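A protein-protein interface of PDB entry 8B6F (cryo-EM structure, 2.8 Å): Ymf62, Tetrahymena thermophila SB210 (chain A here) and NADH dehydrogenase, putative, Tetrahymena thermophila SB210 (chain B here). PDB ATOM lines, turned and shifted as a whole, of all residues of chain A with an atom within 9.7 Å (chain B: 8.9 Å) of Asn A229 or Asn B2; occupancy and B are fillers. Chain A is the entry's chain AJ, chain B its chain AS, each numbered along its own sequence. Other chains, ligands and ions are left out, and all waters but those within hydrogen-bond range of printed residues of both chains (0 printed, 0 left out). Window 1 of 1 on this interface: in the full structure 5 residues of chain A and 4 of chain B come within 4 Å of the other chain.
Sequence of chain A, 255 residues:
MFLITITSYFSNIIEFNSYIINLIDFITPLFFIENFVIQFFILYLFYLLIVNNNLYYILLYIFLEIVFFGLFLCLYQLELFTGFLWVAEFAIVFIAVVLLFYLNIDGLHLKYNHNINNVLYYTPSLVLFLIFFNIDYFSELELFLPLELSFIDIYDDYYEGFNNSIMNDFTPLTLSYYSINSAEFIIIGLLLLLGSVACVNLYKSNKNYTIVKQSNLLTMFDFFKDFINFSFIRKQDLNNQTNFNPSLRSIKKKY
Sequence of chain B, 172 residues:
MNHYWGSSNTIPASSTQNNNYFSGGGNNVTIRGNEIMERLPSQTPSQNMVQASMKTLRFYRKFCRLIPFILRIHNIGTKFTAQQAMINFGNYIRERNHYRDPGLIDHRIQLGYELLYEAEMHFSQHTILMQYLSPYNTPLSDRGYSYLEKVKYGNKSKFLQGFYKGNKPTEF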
ATOM      1  N   THR A 210      -8.221  11.472 -28.943  1.00  0.00           N
ATOM      2  CA  THR A 210      -7.811  12.203 -27.749  1.00  0.00           C
ATOM      3  C   THR A 210      -8.051  11.406 -26.473  1.00  0.00           C
ATOM      4  O   THR A 210      -7.436  11.707 -25.447  1.00  0.00           O
ATOM      5  CB  THR A 210      -8.529  13.554 -27.664  1.00  0.00           C
ATOM      6  OG1 THR A 210      -8.195  14.201 -26.429  1.00  0.00           O
ATOM      7  CG2 THR A 210     -10.036  13.396 -27.752  1.00  0.00           C
ATOM      8  N   GLN A 214      -5.532   9.335 -22.244  1.00  0.00           N
ATOM      9  CA  GLN A 214      -5.979   9.935 -20.990  1.00  0.00           C
ATOM     10  C   GLN A 214      -5.789   8.977 -19.822  1.00  0.00           C
ATOM     11  O   GLN A 214      -5.454   9.400 -18.710  1.00  0.00           O
ATOM     12  CB  GLN A 214      -7.442  10.359 -21.102  1.00  0.00           C
ATOM     13  CG  GLN A 214      -7.704  11.323 -22.239  1.00  0.00           C
ATOM     14  CD  GLN A 214      -9.121  11.848 -22.232  1.00  0.00           C
ATOM     15  OE1 GLN A 214      -9.876  11.614 -21.291  1.00  0.00           O
ATOM     16  NE2 GLN A 214      -9.491  12.566 -23.286  1.00  0.00           N
ATOM     17  N   LEU A 217      -2.186   9.110 -18.790  1.00  0.00           N
ATOM     18  CA  LEU A 217      -1.935  10.425 -18.209  1.00  0.00           C
ATOM     19  C   LEU A 217      -2.400  10.472 -16.760  1.00  0.00           C
ATOM     20  O   LEU A 217      -1.644  10.861 -15.863  1.00  0.00           O
ATOM     21  CB  LEU A 217      -2.638  11.503 -19.034  1.00  0.00           C
ATOM     22  CG  LEU A 217      -2.495  12.943 -18.534  1.00  0.00           C
ATOM     23  CD1 LEU A 217      -1.057  13.411 -18.645  1.00  0.00           C
ATOM     24  CD2 LEU A 217      -3.419  13.869 -19.300  1.00  0.00           C
ATOM     25  N   LEU A 218      -3.650  10.082 -16.511  1.00  0.00           N
ATOM     26  CA  LEU A 218      -4.189  10.147 -15.158  1.00  0.00           C
ATOM     27  C   LEU A 218      -3.555   9.107 -14.246  1.00  0.00           C
ATOM     28  O   LEU A 218      -3.517   9.297 -13.026  1.00  0.00           O
ATOM     29  CB  LEU A 218      -5.707   9.972 -15.191  1.00  0.00           C
ATOM     30  CG  LEU A 218      -6.482  11.042 -15.965  1.00  0.00           C
ATOM     31  CD1 LEU A 218      -7.955  10.688 -16.033  1.00  0.00           C
ATOM     32  CD2 LEU A 218      -6.293  12.414 -15.338  1.00  0.00           C
ATOM     33  N   PHE A 221       0.372  10.669 -13.708  1.00  0.00           N
ATOM     34  CA  PHE A 221       0.483  12.040 -13.230  1.00  0.00           C
ATOM     35  C   PHE A 221      -0.620  12.321 -12.221  1.00  0.00           C
ATOM     36  O   PHE A 221      -1.788  12.006 -12.467  1.00  0.00           O
ATOM     37  CB  PHE A 221       0.403  13.033 -14.392  1.00  0.00           C
ATOM     38  CG  PHE A 221       1.587  12.978 -15.312  1.00  0.00           C
ATOM     39  CD1 PHE A 221       2.698  13.769 -15.076  1.00  0.00           C
ATOM     40  CD2 PHE A 221       1.590  12.132 -16.407  1.00  0.00           C
ATOM     41  CE1 PHE A 221       3.792  13.718 -15.919  1.00  0.00           C
ATOM     42  CE2 PHE A 221       2.679  12.075 -17.254  1.00  0.00           C
ATOM     43  CZ  PHE A 221       3.782  12.869 -17.010  1.00  0.00           C
ATOM     44  N   ASP A 222      -0.245  12.912 -11.090  1.00  0.00           N
ATOM     45  CA  ASP A 222      -1.222  13.272 -10.072  1.00  0.00           C
ATOM     46  C   ASP A 222      -2.080  14.430 -10.564  1.00  0.00           C
ATOM     47  O   ASP A 222      -1.560  15.465 -10.987  1.00  0.00           O
ATOM     48  CB  ASP A 222      -0.518  13.653  -8.772  1.00  0.00           C
ATOM     49  CG  ASP A 222       0.380  12.549  -8.254  1.00  0.00           C
ATOM     50  OD1 ASP A 222       0.069  11.364  -8.495  1.00  0.00           O
ATOM     51  OD2 ASP A 222       1.400  12.867  -7.607  1.00  0.00           O
ATOM     52  N   PHE A 223      -3.400  14.258 -10.502  1.00  0.00           N
ATOM     53  CA  PHE A 223      -4.297  15.289 -11.004  1.00  0.00           C
ATOM     54  C   PHE A 223      -4.282  16.539 -10.136  1.00  0.00           C
ATOM     55  O   PHE A 223      -4.662  17.613 -10.614  1.00  0.00           O
ATOM     56  CB  PHE A 223      -5.720  14.744 -11.105  1.00  0.00           C
ATOM     57  CG  PHE A 223      -6.682  15.692 -11.753  1.00  0.00           C
ATOM     58  CD1 PHE A 223      -6.584  15.977 -13.103  1.00  0.00           C
ATOM     59  CD2 PHE A 223      -7.687  16.293 -11.017  1.00  0.00           C
ATOM     60  CE1 PHE A 223      -7.465  16.850 -13.708  1.00  0.00           C
ATOM     61  CE2 PHE A 223      -8.575  17.166 -11.615  1.00  0.00           C
ATOM     62  CZ  PHE A 223      -8.463  17.444 -12.963  1.00  0.00           C
ATOM     63  N   ASP A 226       0.410  17.550  -9.586  1.00  0.00           N
ATOM     64  CA  ASP A 226       1.061  17.946 -10.827  1.00  0.00           C
ATOM     65  C   ASP A 226       0.183  18.918 -11.603  1.00  0.00           C
ATOM     66  O   ASP A 226      -1.040  18.764 -11.660  1.00  0.00           O
ATOM     67  CB  ASP A 226       1.370  16.722 -11.692  1.00  0.00           C
ATOM     68  CG  ASP A 226       2.366  15.786 -11.038  1.00  0.00           C
ATOM     69  OD1 ASP A 226       3.279  16.276 -10.343  1.00  0.00           O
ATOM     70  OD2 ASP A 226       2.236  14.558 -11.218  1.00  0.00           O
ATOM     71  N   PHE A 227       0.821  19.919 -12.206  1.00  0.00           N
ATOM     72  CA  PHE A 227       0.122  20.966 -12.949  1.00  0.00           C
ATOM     73  C   PHE A 227       0.063  20.539 -14.409  1.00  0.00           C
ATOM     74  O   PHE A 227       0.988  20.769 -15.186  1.00  0.00           O
ATOM     75  CB  PHE A 227       0.829  22.305 -12.769  1.00  0.00           C
ATOM     76  CG  PHE A 227       0.098  23.466 -13.376  1.00  0.00           C
ATOM     77  CD1 PHE A 227      -1.172  23.806 -12.942  1.00  0.00           C
ATOM     78  CD2 PHE A 227       0.694  24.238 -14.357  1.00  0.00           C
ATOM     79  CE1 PHE A 227      -1.841  24.881 -13.490  1.00  0.00           C
ATOM     80  CE2 PHE A 227       0.030  25.315 -14.910  1.00  0.00           C
ATOM     81  CZ  PHE A 227      -1.240  25.638 -14.475  1.00  0.00           C
ATOM     82  N   ILE A 228      -1.048  19.910 -14.787  1.00  0.00           N
ATOM     83  CA  ILE A 228      -1.249  19.383 -16.132  1.00  0.00           C
ATOM     84  C   ILE A 228      -2.226  20.290 -16.864  1.00  0.00           C
ATOM     85  O   ILE A 228      -3.272  20.658 -16.319  1.00  0.00           O
ATOM     86  CB  ILE A 228      -1.759  17.930 -16.104  1.00  0.00           C
ATOM     87  CG1 ILE A 228      -3.107  17.848 -15.379  1.00  0.00           C
ATOM     88  CG2 ILE A 228      -0.718  17.029 -15.449  1.00  0.00           C
ATOM     89  CD1 ILE A 228      -3.652  16.443 -15.231  1.00  0.00           C
ATOM     90  N   ASN A 229      -1.879  20.657 -18.094  1.00  0.00           N
ATOM     91  CA  ASN A 229      -2.733  21.512 -18.901  1.00  0.00           C
ATOM     92  C   ASN A 229      -3.900  20.718 -19.468  1.00  0.00           C
ATOM     93  O   ASN A 229      -3.742  19.573 -19.900  1.00  0.00           O
ATOM     94  CB  ASN A 229      -1.929  22.140 -20.040  1.00  0.00           C
ATOM     95  CG  ASN A 229      -2.772  23.038 -20.918  1.00  0.00           C
ATOM     96  OD1 ASN A 229      -3.794  23.566 -20.484  1.00  0.00           O
ATOM     97  ND2 ASN A 229      -2.347  23.216 -22.162  1.00  0.00           N
ATOM     98  N   PHE A 230      -5.080  21.332 -19.461  1.00  0.00           N
ATOM     99  CA  PHE A 230      -6.258  20.717 -20.051  1.00  0.00           C
ATOM    100  C   PHE A 230      -7.275  21.806 -20.353  1.00  0.00           C
ATOM    101  O   PHE A 230      -7.192  22.921 -19.834  1.00  0.00           O
ATOM    102  CB  PHE A 230      -6.864  19.652 -19.129  1.00  0.00           C
ATOM    103  CG  PHE A 230      -7.396  20.199 -17.838  1.00  0.00           C
ATOM    104  CD1 PHE A 230      -6.569  20.343 -16.738  1.00  0.00           C
ATOM    105  CD2 PHE A 230      -8.728  20.558 -17.720  1.00  0.00           C
ATOM    106  CE1 PHE A 230      -7.056  20.842 -15.548  1.00  0.00           C
ATOM    107  CE2 PHE A 230      -9.223  21.058 -16.535  1.00  0.00           C
ATOM    108  CZ  PHE A 230      -8.386  21.200 -15.447  1.00  0.00           C
ATOM    109  N   SER A 231      -8.233  21.464 -21.208  1.00  0.00           N
ATOM    110  CA  SER A 231      -9.324  22.355 -21.567  1.00  0.00           C
ATOM    111  C   SER A 231     -10.644  21.631 -21.350  1.00  0.00           C
ATOM    112  O   SER A 231     -10.728  20.410 -21.500  1.00  0.00           O
ATOM    113  CB  SER A 231      -9.207  22.820 -23.023  1.00  0.00           C
ATOM    114  OG  SER A 231     -10.267  23.692 -23.372  1.00  0.00           O
ATOM    115  N   PHE A 232     -11.676  22.392 -20.992  1.00  0.00           N
ATOM    116  CA  PHE A 232     -12.973  21.800 -20.710  1.00  0.00           C
ATOM    117  C   PHE A 232     -14.072  22.804 -21.023  1.00  0.00           C
ATOM    118  O   PHE A 232     -13.833  24.009 -21.124  1.00  0.00           O
ATOM    119  CB  PHE A 232     -13.075  21.334 -19.253  1.00  0.00           C
ATOM    120  CG  PHE A 232     -13.036  22.453 -18.256  1.00  0.00           C
ATOM    121  CD1 PHE A 232     -11.831  23.008 -17.864  1.00  0.00           C
ATOM    122  CD2 PHE A 232     -14.207  22.943 -17.705  1.00  0.00           C
ATOM    123  CE1 PHE A 232     -11.794  24.037 -16.947  1.00  0.00           C
ATOM    124  CE2 PHE A 232     -14.177  23.973 -16.787  1.00  0.00           C
ATOM    125  CZ  PHE A 232     -12.969  24.520 -16.408  1.00  0.00           C
ATOM    126  N   MET B   1       5.438  20.000 -21.369  1.00  0.00           N
ATOM    127  CA  MET B   1       5.722  21.006 -20.306  1.00  0.00           C
ATOM    128  C   MET B   1       4.648  22.086 -20.308  1.00  0.00           C
ATOM    129  O   MET B   1       4.386  22.706 -21.336  1.00  0.00           O
ATOM    130  CB  MET B   1       7.101  21.631 -20.517  1.00  0.00           C
ATOM    131  CG  MET B   1       7.643  22.363 -19.304  1.00  0.00           C
ATOM    132  SD  MET B   1       8.062  21.254 -17.947  1.00  0.00           S
ATOM    133  CE  MET B   1       8.691  22.417 -16.741  1.00  0.00           C
ATOM    134  N   ASN B   2       4.026  22.312 -19.150  1.00  0.00           N
ATOM    135  CA  ASN B   2       2.929  23.275 -19.035  1.00  0.00           C
ATOM    136  C   ASN B   2       3.520  24.637 -18.687  1.00  0.00           C
ATOM    137  O   ASN B   2       3.445  25.122 -17.557  1.00  0.00           O
ATOM    138  CB  ASN B   2       1.917  22.808 -17.998  1.00  0.00           C
ATOM    139  CG  ASN B   2       0.656  23.644 -18.001  1.00  0.00           C
ATOM    140  OD1 ASN B   2       0.533  24.599 -18.765  1.00  0.00           O
ATOM    141  ND2 ASN B   2      -0.298  23.275 -17.158  1.00  0.00           N
ATOM    142  N   HIS B   3       4.120  25.261 -19.697  1.00  0.00           N
ATOM    143  CA  HIS B   3       4.746  26.564 -19.546  1.00  0.00           C
ATOM    144  C   HIS B   3       4.680  27.276 -20.887  1.00  0.00           C
ATOM    145  O   HIS B   3       4.503  26.648 -21.933  1.00  0.00           O
ATOM    146  CB  HIS B   3       6.196  26.429 -19.069  1.00  0.00           C
ATOM    147  CG  HIS B   3       6.777  27.693 -18.517  1.00  0.00           C
ATOM    148  ND1 HIS B   3       7.284  28.693 -19.318  1.00  0.00           N
ATOM    149  CD2 HIS B   3       6.942  28.113 -17.242  1.00  0.00           C
ATOM    150  CE1 HIS B   3       7.730  29.677 -18.560  1.00  0.00           C
ATOM    151  NE2 HIS B   3       7.536  29.350 -17.295  1.00  0.00           N
ATOM    152  N   TYR B   4       4.820  28.602 -20.850  1.00  0.00           N
ATOM    153  CA  TYR B   4       4.769  29.369 -22.090  1.00  0.00           C
ATOM    154  C   TYR B   4       5.906  28.991 -23.030  1.00  0.00           C
ATOM    155  O   TYR B   4       5.748  29.062 -24.254  1.00  0.00           O
ATOM    156  CB  TYR B   4       4.810  30.865 -21.786  1.00  0.00           C
ATOM    157  CG  TYR B   4       4.792  31.721 -23.027  1.00  0.00           C
ATOM    158  CD1 TYR B   4       3.630  31.876 -23.770  1.00  0.00           C
ATOM    159  CD2 TYR B   4       5.935  32.378 -23.455  1.00  0.00           C
ATOM    160  CE1 TYR B   4       3.610  32.657 -24.906  1.00  0.00           C
ATOM    161  CE2 TYR B   4       5.925  33.162 -24.589  1.00  0.00           C
ATOM    162  CZ  TYR B   4       4.759  33.298 -25.310  1.00  0.00           C
ATOM    163  OH  TYR B   4       4.746  34.077 -26.441  1.00  0.00           O
ATOM    164  N   TRP B   5       7.050  28.592 -22.485  1.00  0.00           N
ATOM    165  CA  TRP B   5       8.208  28.196 -23.271  1.00  0.00           C
ATOM    166  C   TRP B   5       8.243  26.700 -23.556  1.00  0.00           C
ATOM    167  O   TRP B   5       9.224  26.214 -24.126  1.00  0.00           O
ATOM    168  CB  TRP B   5       9.490  28.610 -22.550  1.00  0.00           C
ATOM    169  CG  TRP B   5       9.670  30.091 -22.447  1.00  0.00           C
ATOM    170  CD1 TRP B   5       9.267  31.031 -23.349  1.00  0.00           C
ATOM    171  CD2 TRP B   5      10.296  30.805 -21.377  1.00  0.00           C
ATOM    172  NE1 TRP B   5       9.606  32.285 -22.909  1.00  0.00           N
ATOM    173  CE2 TRP B   5      10.242  32.174 -21.701  1.00  0.00           C
ATOM    174  CE3 TRP B   5      10.904  30.419 -20.179  1.00  0.00           C
ATOM    175  CZ2 TRP B   5      10.767  33.157 -20.868  1.00  0.00           C
ATOM    176  CZ3 TRP B   5      11.426  31.396 -19.354  1.00  0.00           C
ATOM    177  CH2 TRP B   5      11.354  32.750 -19.702  1.00  0.00           C
ATOM    178  N   GLY B   6       7.204  25.964 -23.173  1.00  0.00           N
ATOM    179  CA  GLY B   6       7.207  24.533 -23.394  1.00  0.00           C
ATOM    180  C   GLY B   6       7.248  24.190 -24.870  1.00  0.00           C
ATOM    181  O   GLY B   6       6.815  24.961 -25.727  1.00  0.00           O
ATOM    182  N   SER B   7       7.779  23.004 -25.165  1.00  0.00           N
ATOM    183  CA  SER B   7       7.916  22.556 -26.544  1.00  0.00           C
ATOM    184  C   SER B   7       6.575  22.298 -27.218  1.00  0.00           C
ATOM    185  O   SER B   7       6.539  22.163 -28.445  1.00  0.00           O
ATOM    186  CB  SER B   7       8.772  21.292 -26.600  1.00  0.00           C
ATOM    187  OG  SER B   7       8.216  20.261 -25.805  1.00  0.00           O
ATOM    188  N   SER B   8       5.486  22.222 -26.458  1.00  0.00           N
ATOM    189  CA  SER B   8       4.159  21.999 -27.013  1.00  0.00           C
ATOM    190  C   SER B   8       3.381  23.291 -27.216  1.00  0.00           C
ATOM    191  O   SER B   8       2.226  23.239 -27.646  1.00  0.00           O
ATOM    192  CB  SER B   8       3.359  21.061 -26.103  1.00  0.00           C
ATOM    193  OG  SER B   8       3.959  19.779 -26.037  1.00  0.00           O
ATOM    194  N   ASN B   9       3.982  24.442 -26.926  1.00  0.00           N
ATOM    195  CA  ASN B   9       3.335  25.732 -27.109  1.00  0.00           C
ATOM    196  C   ASN B   9       3.594  26.320 -28.490  1.00  0.00           C
ATOM    197  O   ASN B   9       3.398  27.522 -28.693  1.00  0.00           O
ATOM    198  CB  ASN B   9       3.800  26.705 -26.024  1.00  0.00           C
ATOM    199  CG  ASN B   9       2.942  27.949 -25.948  1.00  0.00           C
ATOM    200  OD1 ASN B   9       1.793  27.951 -26.383  1.00  0.00           O
ATOM    201  ND2 ASN B   9       3.495  29.017 -25.390  1.00  0.00           N
ATOM    202  N   GLU B  35      -0.189  29.608 -27.103  1.00  0.00           N
ATOM    203  CA  GLU B  35      -1.009  30.023 -25.975  1.00  0.00           C
ATOM    204  C   GLU B  35      -0.344  31.177 -25.234  1.00  0.00           C
ATOM    205  O   GLU B  35       0.884  31.266 -25.157  1.00  0.00           O
ATOM    206  CB  GLU B  35      -1.238  28.855 -25.015  1.00  0.00           C
ATOM    207  CG  GLU B  35      -1.773  27.600 -25.684  1.00  0.00           C
ATOM    208  CD  GLU B  35      -2.117  26.510 -24.686  1.00  0.00           C
ATOM    209  OE1 GLU B  35      -2.759  26.822 -23.663  1.00  0.00           O
ATOM    210  OE2 GLU B  35      -1.741  25.342 -24.920  1.00  0.00           O
ATOM    211  N   ILE B  36      -1.171  32.062 -24.680  1.00  0.00           N
ATOM    212  CA  ILE B  36      -0.672  33.229 -23.960  1.00  0.00           C
ATOM    213  C   ILE B  36      -0.050  32.781 -22.645  1.00  0.00           C
ATOM    214  O   ILE B  36      -0.253  31.646 -22.202  1.00  0.00           O
ATOM    215  CB  ILE B  36      -1.787  34.263 -23.715  1.00  0.00           C
ATOM    216  CG1 ILE B  36      -2.900  33.661 -22.850  1.00  0.00           C
ATOM    217  CG2 ILE B  36      -2.334  34.758 -25.047  1.00  0.00           C
ATOM    218  CD1 ILE B  36      -3.993  34.643 -22.476  1.00  0.00           C
ATOM    219  N   GLU B  38      -0.075  32.654 -18.954  1.00  0.00           N
ATOM    220  CA  GLU B  38      -0.984  32.834 -17.829  1.00  0.00           C
ATOM    221  C   GLU B  38      -0.250  32.991 -16.508  1.00  0.00           C
ATOM    222  O   GLU B  38      -0.788  33.602 -15.578  1.00  0.00           O
ATOM    223  CB  GLU B  38      -1.950  31.648 -17.741  1.00  0.00           C
ATOM    224  CG  GLU B  38      -3.241  31.937 -16.987  1.00  0.00           C
ATOM    225  CD  GLU B  38      -3.081  31.882 -15.478  1.00  0.00           C
ATOM    226  OE1 GLU B  38      -2.083  31.300 -15.001  1.00  0.00           O
ATOM    227  OE2 GLU B  38      -3.957  32.420 -14.769  1.00  0.00           O
ATOM    228  N   ARG B  39       0.963  32.457 -16.400  1.00  0.00           N
ATOM    229  CA  ARG B  39       1.731  32.542 -15.169  1.00  0.00           C
ATOM    230  C   ARG B  39       3.208  32.431 -15.508  1.00  0.00           C
ATOM    231  O   ARG B  39       3.596  31.634 -16.364  1.00  0.00           O
ATOM    232  CB  ARG B  39       1.322  31.443 -14.179  1.00  0.00           C
ATOM    233  CG  ARG B  39       1.420  30.036 -14.746  1.00  0.00           C
ATOM    234  CD  ARG B  39       0.555  29.052 -13.970  1.00  0.00           C
ATOM    235  NE  ARG B  39       1.097  28.744 -12.652  1.00  0.00           N
ATOM    236  CZ  ARG B  39       0.478  28.003 -11.744  1.00  0.00           C
ATOM    237  NH1 ARG B  39      -0.720  27.492 -11.968  1.00  0.00           N
ATOM    238  NH2 ARG B  39       1.078  27.765 -10.582  1.00  0.00           N
ATOM    239  N   LEU B  40       4.024  33.245 -14.837  1.00  0.00           N
ATOM    240  CA  LEU B  40       5.475  33.247 -15.011  1.00  0.00           C
ATOM    241  C   LEU B  40       6.105  32.999 -13.649  1.00  0.00           C
ATOM    242  O   LEU B  40       6.373  33.951 -12.898  1.00  0.00           O
ATOM    243  CB  LEU B  40       5.954  34.568 -15.607  1.00  0.00           C
ATOM    244  CG  LEU B  40       7.455  34.680 -15.885  1.00  0.00           C
ATOM    245  CD1 LEU B  40       7.915  33.615 -16.867  1.00  0.00           C
ATOM    246  CD2 LEU B  40       7.798  36.067 -16.399  1.00  0.00           C
ATOM    247  N   PRO B  41       6.355  31.744 -13.282  1.00  0.00           N
ATOM    248  CA  PRO B  41       6.901  31.472 -11.949  1.00  0.00           C
ATOM    249  C   PRO B  41       8.238  32.164 -11.733  1.00  0.00           C
ATOM    250  O   PRO B  41       9.017  32.372 -12.665  1.00  0.00           O
ATOM    251  CB  PRO B  41       7.054  29.947 -11.932  1.00  0.00           C
ATOM    252  CG  PRO B  41       6.092  29.459 -12.944  1.00  0.00           C
ATOM    253  CD  PRO B  41       6.053  30.503 -14.014  1.00  0.00           C
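The backbone carbonyl oxygen (O) of Phe A227 lies close to the side-chain amide nitrogen (ND2) of Asn B2.
ND2 of Asn B2 lies close to N of Asn A229, 3.2 Å away.
The side-chain amide oxygen of Asn B9 sits at hydrogen-bond distance from the backbone NH of Glu B35, at 2.7 Å.
Phe A227 touches Arg B39 (CZ to NH1, 3.2 Å).
C of Ile A228 touches ND2 of Asn B2, at 3.6 Å.
OE2 of Glu B35 touches ND2 of Asn A229, 3.5 Å away.
Of chain A, only Phe A227, Ile A228 and Asn A229 come within 4 Å of Asn B2.
No residue of chain A comes within 4 Å of Met B1.
Of the printed residues of chain B, Ile A228 touches Asn B2 (3.6 Å).
Of the printed residues of chain A, Arg B39 touches Phe A227.
Printed residues of chain B within 4 Å of Phe A227: Asn B2 and Arg B39.
Of the printed residues of chain A, Glu B35 touches Asn A229 (3.5 Å).
The nearest residue of chain A that does not touch Asn B2 is Phe A230 (5.7 Å).
Of the 15 printed residues of chain B, 3 touch a printed residue of chain A.
Printed residues of chain B that touch a printed residue of chain A: Asn B2, Glu B35 and Arg B39.
Among the printed residues, 5 pairs touch across the chains.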
